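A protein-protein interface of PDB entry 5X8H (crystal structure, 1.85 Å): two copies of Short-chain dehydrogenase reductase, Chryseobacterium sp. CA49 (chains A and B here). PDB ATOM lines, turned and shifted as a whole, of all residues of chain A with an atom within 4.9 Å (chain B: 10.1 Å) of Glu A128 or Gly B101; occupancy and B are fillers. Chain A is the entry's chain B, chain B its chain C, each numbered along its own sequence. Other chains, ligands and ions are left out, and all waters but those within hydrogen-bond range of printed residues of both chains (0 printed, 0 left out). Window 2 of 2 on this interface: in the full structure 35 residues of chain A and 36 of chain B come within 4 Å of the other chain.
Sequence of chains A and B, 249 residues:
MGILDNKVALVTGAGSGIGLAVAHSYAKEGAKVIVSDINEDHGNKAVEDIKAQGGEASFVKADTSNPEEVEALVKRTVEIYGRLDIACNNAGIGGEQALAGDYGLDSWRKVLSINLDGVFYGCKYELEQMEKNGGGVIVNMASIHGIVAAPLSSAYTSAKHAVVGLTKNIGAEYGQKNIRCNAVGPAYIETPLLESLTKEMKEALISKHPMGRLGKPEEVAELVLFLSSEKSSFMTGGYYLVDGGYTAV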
ATOM      1  N   CYS A 123     -22.833  -2.855   4.151  1.00  0.00           N
ATOM      2  CA  CYS A 123     -22.954  -3.171   2.720  1.00  0.00           C
ATOM      3  C   CYS A 123     -23.264  -4.682   2.478  1.00  0.00           C
ATOM      4  O   CYS A 123     -24.079  -5.016   1.649  1.00  0.00           O
ATOM      5  CB  CYS A 123     -21.662  -2.794   1.955  1.00  0.00           C
ATOM      6  SG  CYS A 123     -21.469  -1.001   1.814  1.00  0.00           S
ATOM      7  N   LYS A 124     -22.558  -5.564   3.163  1.00  0.00           N
ATOM      8  CA  LYS A 124     -22.761  -6.989   3.011  1.00  0.00           C
ATOM      9  C   LYS A 124     -24.245  -7.380   3.223  1.00  0.00           C
ATOM     10  O   LYS A 124     -24.884  -7.982   2.306  1.00  0.00           O
ATOM     11  CB  LYS A 124     -21.834  -7.746   3.958  1.00  0.00           C
ATOM     12  CG  LYS A 124     -21.961  -9.256   3.832  1.00  0.00           C
ATOM     13  CD  LYS A 124     -21.347  -9.946   5.045  1.00  0.00           C
ATOM     14  CE  LYS A 124     -21.464 -11.470   4.961  1.00  0.00           C
ATOM     15  NZ  LYS A 124     -21.273 -12.036   3.603  1.00  0.00           N
ATOM     16  N   TYR A 125     -24.788  -6.974   4.380  1.00  0.00           N
ATOM     17  CA  TYR A 125     -26.141  -7.316   4.764  1.00  0.00           C
ATOM     18  C   TYR A 125     -27.138  -6.475   4.013  1.00  0.00           C
ATOM     19  O   TYR A 125     -28.221  -6.955   3.726  1.00  0.00           O
ATOM     20  CB  TYR A 125     -26.309  -7.253   6.294  1.00  0.00           C
ATOM     21  CG  TYR A 125     -25.389  -8.271   6.938  1.00  0.00           C
ATOM     22  CD1 TYR A 125     -25.483  -9.652   6.624  1.00  0.00           C
ATOM     23  CD2 TYR A 125     -24.408  -7.878   7.810  1.00  0.00           C
ATOM     24  CE1 TYR A 125     -24.595 -10.583   7.195  1.00  0.00           C
ATOM     25  CE2 TYR A 125     -23.537  -8.790   8.393  1.00  0.00           C
ATOM     26  CZ  TYR A 125     -23.630 -10.120   8.091  1.00  0.00           C
ATOM     27  OH  TYR A 125     -22.722 -10.935   8.683  1.00  0.00           O
ATOM     28  N   GLU A 126     -26.761  -5.255   3.605  1.00  0.00           N
ATOM     29  CA  GLU A 126     -27.635  -4.467   2.735  1.00  0.00           C
ATOM     30  C   GLU A 126     -27.739  -5.073   1.362  1.00  0.00           C
ATOM     31  O   GLU A 126     -28.837  -5.174   0.799  1.00  0.00           O
ATOM     32  CB  GLU A 126     -27.180  -3.013   2.618  1.00  0.00           C
ATOM     33  CG  GLU A 126     -27.395  -2.204   3.894  1.00  0.00           C
ATOM     34  CD  GLU A 126     -26.316  -1.154   4.132  1.00  0.00           C
ATOM     35  OE1 GLU A 126     -25.576  -0.806   3.187  1.00  0.00           O
ATOM     36  OE2 GLU A 126     -26.219  -0.686   5.280  1.00  0.00           O
ATOM     37  N   LEU A 127     -26.612  -5.466   0.794  1.00  0.00           N
ATOM     38  CA  LEU A 127     -26.630  -6.014  -0.559  1.00  0.00           C
ATOM     39  C   LEU A 127     -27.492  -7.302  -0.569  1.00  0.00           C
ATOM     40  O   LEU A 127     -28.275  -7.524  -1.489  1.00  0.00           O
ATOM     41  CB  LEU A 127     -25.222  -6.320  -1.019  1.00  0.00           C
ATOM     42  CG  LEU A 127     -24.373  -5.083  -1.377  1.00  0.00           C
ATOM     43  CD1 LEU A 127     -22.933  -5.513  -1.466  1.00  0.00           C
ATOM     44  CD2 LEU A 127     -24.872  -4.471  -2.665  1.00  0.00           C
ATOM     45  N   GLU A 128     -27.290  -8.140   0.418  1.00  0.00           N
ATOM     46  CA  GLU A 128     -28.023  -9.413   0.531  1.00  0.00           C
ATOM     47  C   GLU A 128     -29.522  -9.207   0.382  1.00  0.00           C
ATOM     48  O   GLU A 128     -30.145  -9.813  -0.480  1.00  0.00           O
ATOM     49  CB  GLU A 128     -27.727 -10.099   1.862  1.00  0.00           C
ATOM     50  CG  GLU A 128     -26.522 -11.011   1.824  1.00  0.00           C
ATOM     51  CD  GLU A 128     -26.358 -11.788   3.119  1.00  0.00           C
ATOM     52  OE1 GLU A 128     -27.355 -11.915   3.882  1.00  0.00           O
ATOM     53  OE2 GLU A 128     -25.224 -12.256   3.361  1.00  0.00           O
ATOM     54  N   GLN A 129     -30.056  -8.280   1.164  1.00  0.00           N
ATOM     55  CA  GLN A 129     -31.472  -7.957   1.139  1.00  0.00           C
ATOM     56  C   GLN A 129     -31.932  -7.272  -0.158  1.00  0.00           C
ATOM     57  O   GLN A 129     -33.047  -7.552  -0.652  1.00  0.00           O
ATOM     58  CB  GLN A 129     -31.839  -7.084   2.343  1.00  0.00           C
ATOM     59  CG  GLN A 129     -33.322  -6.764   2.436  1.00  0.00           C
ATOM     60  CD  GLN A 129     -34.204  -8.002   2.231  1.00  0.00           C
ATOM     61  OE1 GLN A 129     -33.883  -9.120   2.696  1.00  0.00           O
ATOM     62  NE2 GLN A 129     -35.279  -7.822   1.469  1.00  0.00           N
ATOM     63  N   MET A 130     -31.094  -6.385  -0.711  1.00  0.00           N
ATOM     64  CA  MET A 130     -31.441  -5.669  -1.941  1.00  0.00           C
ATOM     65  C   MET A 130     -31.533  -6.628  -3.118  1.00  0.00           C
ATOM     66  O   MET A 130     -32.390  -6.440  -3.971  1.00  0.00           O
ATOM     67  CB  MET A 130     -30.424  -4.547  -2.255  1.00  0.00           C
ATOM     68  CG  MET A 130     -30.565  -3.341  -1.346  1.00  0.00           C
ATOM     69  SD  MET A 130     -29.277  -2.074  -1.601  1.00  0.00           S
ATOM     70  CE  MET A 130     -29.909  -0.852  -0.482  1.00  0.00           C
ATOM     71  N   GLU A 131     -30.684  -7.657  -3.168  1.00  0.00           N
ATOM     72  CA  GLU A 131     -30.812  -8.692  -4.213  1.00  0.00           C
ATOM     73  C   GLU A 131     -32.098  -9.520  -4.093  1.00  0.00           C
ATOM     74  O   GLU A 131     -32.509 -10.145  -5.068  1.00  0.00           O
ATOM     75  CB  GLU A 131     -29.610  -9.644  -4.243  1.00  0.00           C
ATOM     76  CG  GLU A 131     -28.298  -8.953  -4.602  1.00  0.00           C
ATOM     77  CD  GLU A 131     -27.519  -9.688  -5.660  1.00  0.00           C
ATOM     78  OE1 GLU A 131     -27.891  -9.581  -6.849  1.00  0.00           O
ATOM     79  OE2 GLU A 131     -26.533 -10.353  -5.290  1.00  0.00           O
ATOM     80  N   LYS A 132     -32.707  -9.548  -2.903  1.00  0.00           N
ATOM     81  CA  LYS A 132     -34.026 -10.185  -2.745  1.00  0.00           C
ATOM     82  C   LYS A 132     -35.172  -9.278  -3.217  1.00  0.00           C
ATOM     83  O   LYS A 132     -36.215  -9.784  -3.631  1.00  0.00           O
ATOM     84  CB  LYS A 132     -34.250 -10.618  -1.295  1.00  0.00           C
ATOM     85  CG  LYS A 132     -33.322 -11.718  -0.804  1.00  0.00           C
ATOM     86  CD  LYS A 132     -33.458 -11.885   0.716  1.00  0.00           C
ATOM     87  CE  LYS A 132     -32.646 -13.066   1.219  1.00  0.00           C
ATOM     88  NZ  LYS A 132     -31.912 -12.743   2.460  1.00  0.00           N
ATOM     89  N   TYR A 174     -21.637  -4.817  -8.797  1.00  0.00           N
ATOM     90  CA  TYR A 174     -23.078  -4.842  -8.843  1.00  0.00           C
ATOM     91  C   TYR A 174     -23.686  -3.959  -9.920  1.00  0.00           C
ATOM     92  O   TYR A 174     -24.891  -3.671  -9.865  1.00  0.00           O
ATOM     93  CB  TYR A 174     -23.645  -4.445  -7.445  1.00  0.00           C
ATOM     94  CG  TYR A 174     -23.387  -5.508  -6.432  1.00  0.00           C
ATOM     95  CD1 TYR A 174     -22.176  -5.621  -5.826  1.00  0.00           C
ATOM     96  CD2 TYR A 174     -24.364  -6.481  -6.139  1.00  0.00           C
ATOM     97  CE1 TYR A 174     -21.888  -6.643  -4.949  1.00  0.00           C
ATOM     98  CE2 TYR A 174     -24.099  -7.518  -5.247  1.00  0.00           C
ATOM     99  CZ  TYR A 174     -22.863  -7.596  -4.634  1.00  0.00           C
ATOM    100  OH  TYR A 174     -22.548  -8.582  -3.712  1.00  0.00           O
ATOM    101  N   GLU B  96      -9.749 -14.243  -0.165  1.00  0.00           N
ATOM    102  CA  GLU B  96     -10.839 -14.928  -0.791  1.00  0.00           C
ATOM    103  C   GLU B  96     -11.339 -14.086  -1.979  1.00  0.00           C
ATOM    104  O   GLU B  96     -11.214 -12.880  -1.963  1.00  0.00           O
ATOM    105  CB  GLU B  96     -11.902 -15.149   0.295  1.00  0.00           C
ATOM    106  CG  GLU B  96     -13.263 -15.583  -0.162  1.00  0.00           C
ATOM    107  CD  GLU B  96     -14.231 -15.693   1.012  1.00  0.00           C
ATOM    108  OE1 GLU B  96     -15.178 -14.878   1.055  1.00  0.00           O
ATOM    109  OE2 GLU B  96     -14.010 -16.578   1.871  1.00  0.00           O
ATOM    110  N   GLN B  97     -11.820 -14.741  -3.027  1.00  0.00           N
ATOM    111  CA  GLN B  97     -12.470 -14.076  -4.175  1.00  0.00           C
ATOM    112  C   GLN B  97     -13.976 -14.341  -4.179  1.00  0.00           C
ATOM    113  O   GLN B  97     -14.411 -15.463  -4.394  1.00  0.00           O
ATOM    114  CB  GLN B  97     -11.827 -14.527  -5.494  1.00  0.00           C
ATOM    115  CG  GLN B  97     -10.328 -14.265  -5.497  1.00  0.00           C
ATOM    116  CD  GLN B  97      -9.648 -14.523  -6.825  1.00  0.00           C
ATOM    117  OE1 GLN B  97     -10.276 -14.485  -7.884  1.00  0.00           O
ATOM    118  NE2 GLN B  97      -8.336 -14.765  -6.772  1.00  0.00           N
ATOM    119  N   ALA B  98     -14.764 -13.306  -3.909  1.00  0.00           N
ATOM    120  CA  ALA B  98     -16.217 -13.397  -3.827  1.00  0.00           C
ATOM    121  C   ALA B  98     -16.801 -12.000  -3.987  1.00  0.00           C
ATOM    122  O   ALA B  98     -16.105 -10.999  -3.695  1.00  0.00           O
ATOM    123  CB  ALA B  98     -16.625 -13.971  -2.471  1.00  0.00           C
ATOM    124  N   LEU B  99     -18.082 -11.916  -4.358  1.00  0.00           N
ATOM    125  CA  LEU B  99     -18.806 -10.629  -4.378  1.00  0.00           C
ATOM    126  C   LEU B  99     -18.786 -10.009  -2.988  1.00  0.00           C
ATOM    127  O   LEU B  99     -18.730 -10.732  -1.992  1.00  0.00           O
ATOM    128  CB  LEU B  99     -20.231 -10.787  -4.920  1.00  0.00           C
ATOM    129  CG  LEU B  99     -20.360 -11.245  -6.381  1.00  0.00           C
ATOM    130  CD1 LEU B  99     -21.776 -11.702  -6.707  1.00  0.00           C
ATOM    131  CD2 LEU B  99     -19.945 -10.139  -7.340  1.00  0.00           C
ATOM    132  N   ALA B 100     -18.791  -8.680  -2.909  1.00  0.00           N
ATOM    133  CA  ALA B 100     -18.750  -8.019  -1.577  1.00  0.00           C
ATOM    134  C   ALA B 100     -19.871  -8.563  -0.658  1.00  0.00           C
ATOM    135  O   ALA B 100     -19.612  -8.939   0.477  1.00  0.00           O
ATOM    136  CB  ALA B 100     -18.844  -6.506  -1.713  1.00  0.00           C
ATOM    137  N   GLY B 101     -21.095  -8.651  -1.176  1.00  0.00           N
ATOM    138  CA  GLY B 101     -22.233  -9.197  -0.398  1.00  0.00           C
ATOM    139  C   GLY B 101     -22.076 -10.655   0.052  1.00  0.00           C
ATOM    140  O   GLY B 101     -22.726 -11.066   0.973  1.00  0.00           O
ATOM    141  N   ASP B 102     -21.196 -11.413  -0.599  1.00  0.00           N
ATOM    142  CA  ASP B 102     -20.890 -12.802  -0.259  1.00  0.00           C
ATOM    143  C   ASP B 102     -19.554 -13.004   0.464  1.00  0.00           C
ATOM    144  O   ASP B 102     -19.174 -14.140   0.729  1.00  0.00           O
ATOM    145  CB  ASP B 102     -20.855 -13.666  -1.530  1.00  0.00           C
ATOM    146  CG  ASP B 102     -22.156 -13.681  -2.262  1.00  0.00           C
ATOM    147  OD1 ASP B 102     -23.229 -13.631  -1.615  1.00  0.00           O
ATOM    148  OD2 ASP B 102     -22.105 -13.740  -3.500  1.00  0.00           O
ATOM    149  N   TYR B 103     -18.840 -11.927   0.778  1.00  0.00           N
ATOM    150  CA  TYR B 103     -17.488 -12.022   1.278  1.00  0.00           C
ATOM    151  C   TYR B 103     -17.587 -12.501   2.729  1.00  0.00           C
ATOM    152  O   TYR B 103     -18.396 -11.958   3.513  1.00  0.00           O
ATOM    153  CB  TYR B 103     -16.753 -10.644   1.162  1.00  0.00           C
ATOM    154  CG  TYR B 103     -15.284 -10.790   0.878  1.00  0.00           C
ATOM    155  CD1 TYR B 103     -14.368 -10.887   1.895  1.00  0.00           C
ATOM    156  CD2 TYR B 103     -14.820 -10.875  -0.422  1.00  0.00           C
ATOM    157  CE1 TYR B 103     -13.025 -11.071   1.643  1.00  0.00           C
ATOM    158  CE2 TYR B 103     -13.471 -11.078  -0.683  1.00  0.00           C
ATOM    159  CZ  TYR B 103     -12.584 -11.192   0.367  1.00  0.00           C
ATOM    160  OH  TYR B 103     -11.259 -11.395   0.143  1.00  0.00           O
ATOM    161  N   GLY B 104     -16.783 -13.509   3.082  1.00  0.00           N
ATOM    162  CA  GLY B 104     -16.702 -14.006   4.481  1.00  0.00           C
ATOM    163  C   GLY B 104     -16.226 -12.971   5.487  1.00  0.00           C
ATOM    164  O   GLY B 104     -15.291 -12.151   5.197  1.00  0.00           O
ATOM    165  N   LEU B 105     -16.836 -13.004   6.675  1.00  0.00           N
ATOM    166  CA  LEU B 105     -16.452 -12.108   7.746  1.00  0.00           C
ATOM    167  C   LEU B 105     -15.020 -12.348   8.168  1.00  0.00           C
ATOM    168  O   LEU B 105     -14.235 -11.377   8.332  1.00  0.00           O
ATOM    169  CB  LEU B 105     -17.377 -12.272   8.952  1.00  0.00           C
ATOM    170  CG  LEU B 105     -18.849 -11.908   8.751  1.00  0.00           C
ATOM    171  CD1 LEU B 105     -19.683 -12.195  10.002  1.00  0.00           C
ATOM    172  CD2 LEU B 105     -19.004 -10.443   8.349  1.00  0.00           C
ATOM    173  N   TRP B 108     -12.503 -11.254   5.260  1.00  0.00           N
ATOM    174  CA  TRP B 108     -12.391  -9.789   5.313  1.00  0.00           C
ATOM    175  C   TRP B 108     -11.397  -9.404   6.384  1.00  0.00           C
ATOM    176  O   TRP B 108     -10.434  -8.715   6.109  1.00  0.00           O
ATOM    177  CB  TRP B 108     -13.714  -9.130   5.612  1.00  0.00           C
ATOM    178  CG  TRP B 108     -13.630  -7.641   5.807  1.00  0.00           C
ATOM    179  CD1 TRP B 108     -13.450  -6.966   6.966  1.00  0.00           C
ATOM    180  CD2 TRP B 108     -13.712  -6.658   4.779  1.00  0.00           C
ATOM    181  NE1 TRP B 108     -13.427  -5.600   6.726  1.00  0.00           N
ATOM    182  CE2 TRP B 108     -13.612  -5.391   5.389  1.00  0.00           C
ATOM    183  CE3 TRP B 108     -13.923  -6.727   3.408  1.00  0.00           C
ATOM    184  CZ2 TRP B 108     -13.649  -4.193   4.657  1.00  0.00           C
ATOM    185  CZ3 TRP B 108     -13.972  -5.535   2.675  1.00  0.00           C
ATOM    186  CH2 TRP B 108     -13.841  -4.291   3.303  1.00  0.00           C
ATOM    187  N   LEU B 152     -14.361  -8.805  -7.044  1.00  0.00           N
ATOM    188  CA  LEU B 152     -14.249 -10.037  -6.247  1.00  0.00           C
ATOM    189  C   LEU B 152     -13.186 -10.010  -5.152  1.00  0.00           C
ATOM    190  O   LEU B 152     -13.015 -10.984  -4.410  1.00  0.00           O
ATOM    191  CB  LEU B 152     -14.067 -11.295  -7.135  1.00  0.00           C
ATOM    192  CG  LEU B 152     -15.051 -11.447  -8.288  1.00  0.00           C
ATOM    193  CD1 LEU B 152     -14.762 -12.766  -9.007  1.00  0.00           C
ATOM    194  CD2 LEU B 152     -16.517 -11.343  -7.859  1.00  0.00           C
ATOM    195  N   SER B 153     -12.426  -8.925  -5.063  1.00  0.00           N
ATOM    196  CA  SER B 153     -11.418  -8.787  -4.030  1.00  0.00           C
ATOM    197  C   SER B 153     -11.608  -7.444  -3.265  1.00  0.00           C
ATOM    198  O   SER B 153     -10.670  -6.651  -3.139  1.00  0.00           O
ATOM    199  CB  SER B 153     -10.041  -8.825  -4.684  1.00  0.00           C
ATOM    200  OG  SER B 153      -9.775 -10.047  -5.321  1.00  0.00           O
ATOM    201  N   SER B 154     -12.810  -7.214  -2.748  1.00  0.00           N
ATOM    202  CA  SER B 154     -13.143  -5.971  -2.041  1.00  0.00           C
ATOM    203  C   SER B 154     -12.293  -5.752  -0.791  1.00  0.00           C
ATOM    204  O   SER B 154     -11.841  -4.607  -0.531  1.00  0.00           O
ATOM    205  CB  SER B 154     -14.634  -5.915  -1.747  1.00  0.00           C
ATOM    206  OG  SER B 154     -14.950  -6.959  -0.873  1.00  0.00           O
ATOM    207  N   ALA B 155     -11.981  -6.833  -0.067  1.00  0.00           N
ATOM    208  CA  ALA B 155     -11.170  -6.696   1.122  1.00  0.00           C
ATOM    209  C   ALA B 155      -9.757  -6.194   0.733  1.00  0.00           C
ATOM    210  O   ALA B 155      -9.215  -5.283   1.357  1.00  0.00           O
ATOM    211  CB  ALA B 155     -11.086  -7.992   1.877  1.00  0.00           C
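Of chain B, only Gly B101 (3.2 Å), Asp B102 (3.7 Å) and Tyr B103 (2.9 Å) come within 4 Å of Lys A124. Of the printed residues of chain B, Tyr A125 touches Leu B105. Glu A128 touches just one residue of chain B: Gly B101. No residue of chain B comes within 4 Å of Gln A129. Printed residues of chain A within 4 Å of Ala B100: Tyr A174. Of the printed residues of chain A, Gly B101 touches Lys A124, Leu A127, Glu A128 and Tyr A174. Printed residues of chain A within 4 Å of Asp B102: Lys A124. Of the printed residues of chain A, Tyr B103 touches Lys A124 (2.9 Å). Of the printed residues of chain A, Leu B105 touches Tyr A125. Ala B155 touches none of the printed residues of chain A. The nearest printed residue of chain A that does not touch Gly B101 is Cys A123 (5.0 Å). The nearest printed residue of chain A that does not touch Leu B105 is Lys A124 (4.1 Å).
Printed residues of chain A that touch a printed residue of chain B: Lys A124, Tyr A125, Leu A127, Glu A128 and Tyr A174. Hydrophobic or aromatic side chains of chain A that line the printed part of chain B: Tyr A125, Leu A127 and Tyr A174. Printed residues of chain B that touch a printed residue of chain A: Leu B99, Ala B100, Gly B101, Asp B102, Tyr B103 and Leu B105. Among the printed residues, 9 pairs touch across the chains. Among the printed residues, no Asp or Glu carboxylate lies within 4 Å of a Lys or Arg side-chain nitrogen of the other chain.
Asp B102 touches Lys A124 (C to NZ, 3.7 Å). Leu B105 touches Tyr A125 (CD1 to OH, 3.5 Å). CD1 of Leu A127 touches N of Gly B101 (3.6 Å). Gly B101 touches Glu A128 (O to OE2, 3.7 Å). Tyr A174 touches Leu B99. OH of Tyr A174 touches N of Ala B100, at 3.8 Å.
NZ of Lys A124 lies within salt-bridge range of OE2 of Glu A128 (3.96 Å). The side-chain hydroxyl (OH) of Tyr B103 lies within hydrogen-bond range of the backbone carbonyl oxygen (O) of Glu B96, 2.6 Å away.
OH of Tyr A174 is in hydrogen-bond range of N of Gly B101, 2.9 Å away. The backbone carbonyl oxygen (O) of Gly B101 sits at hydrogen-bond distance from the side-chain amino group (NZ) of Lys A124 (3.2 Å). The side-chain amino group (NZ) of Lys A124 lies within hydrogen-bond range of the backbone carbonyl oxygen (O) of Tyr B103, 2.9 Å away.
No position is printed for both chains.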
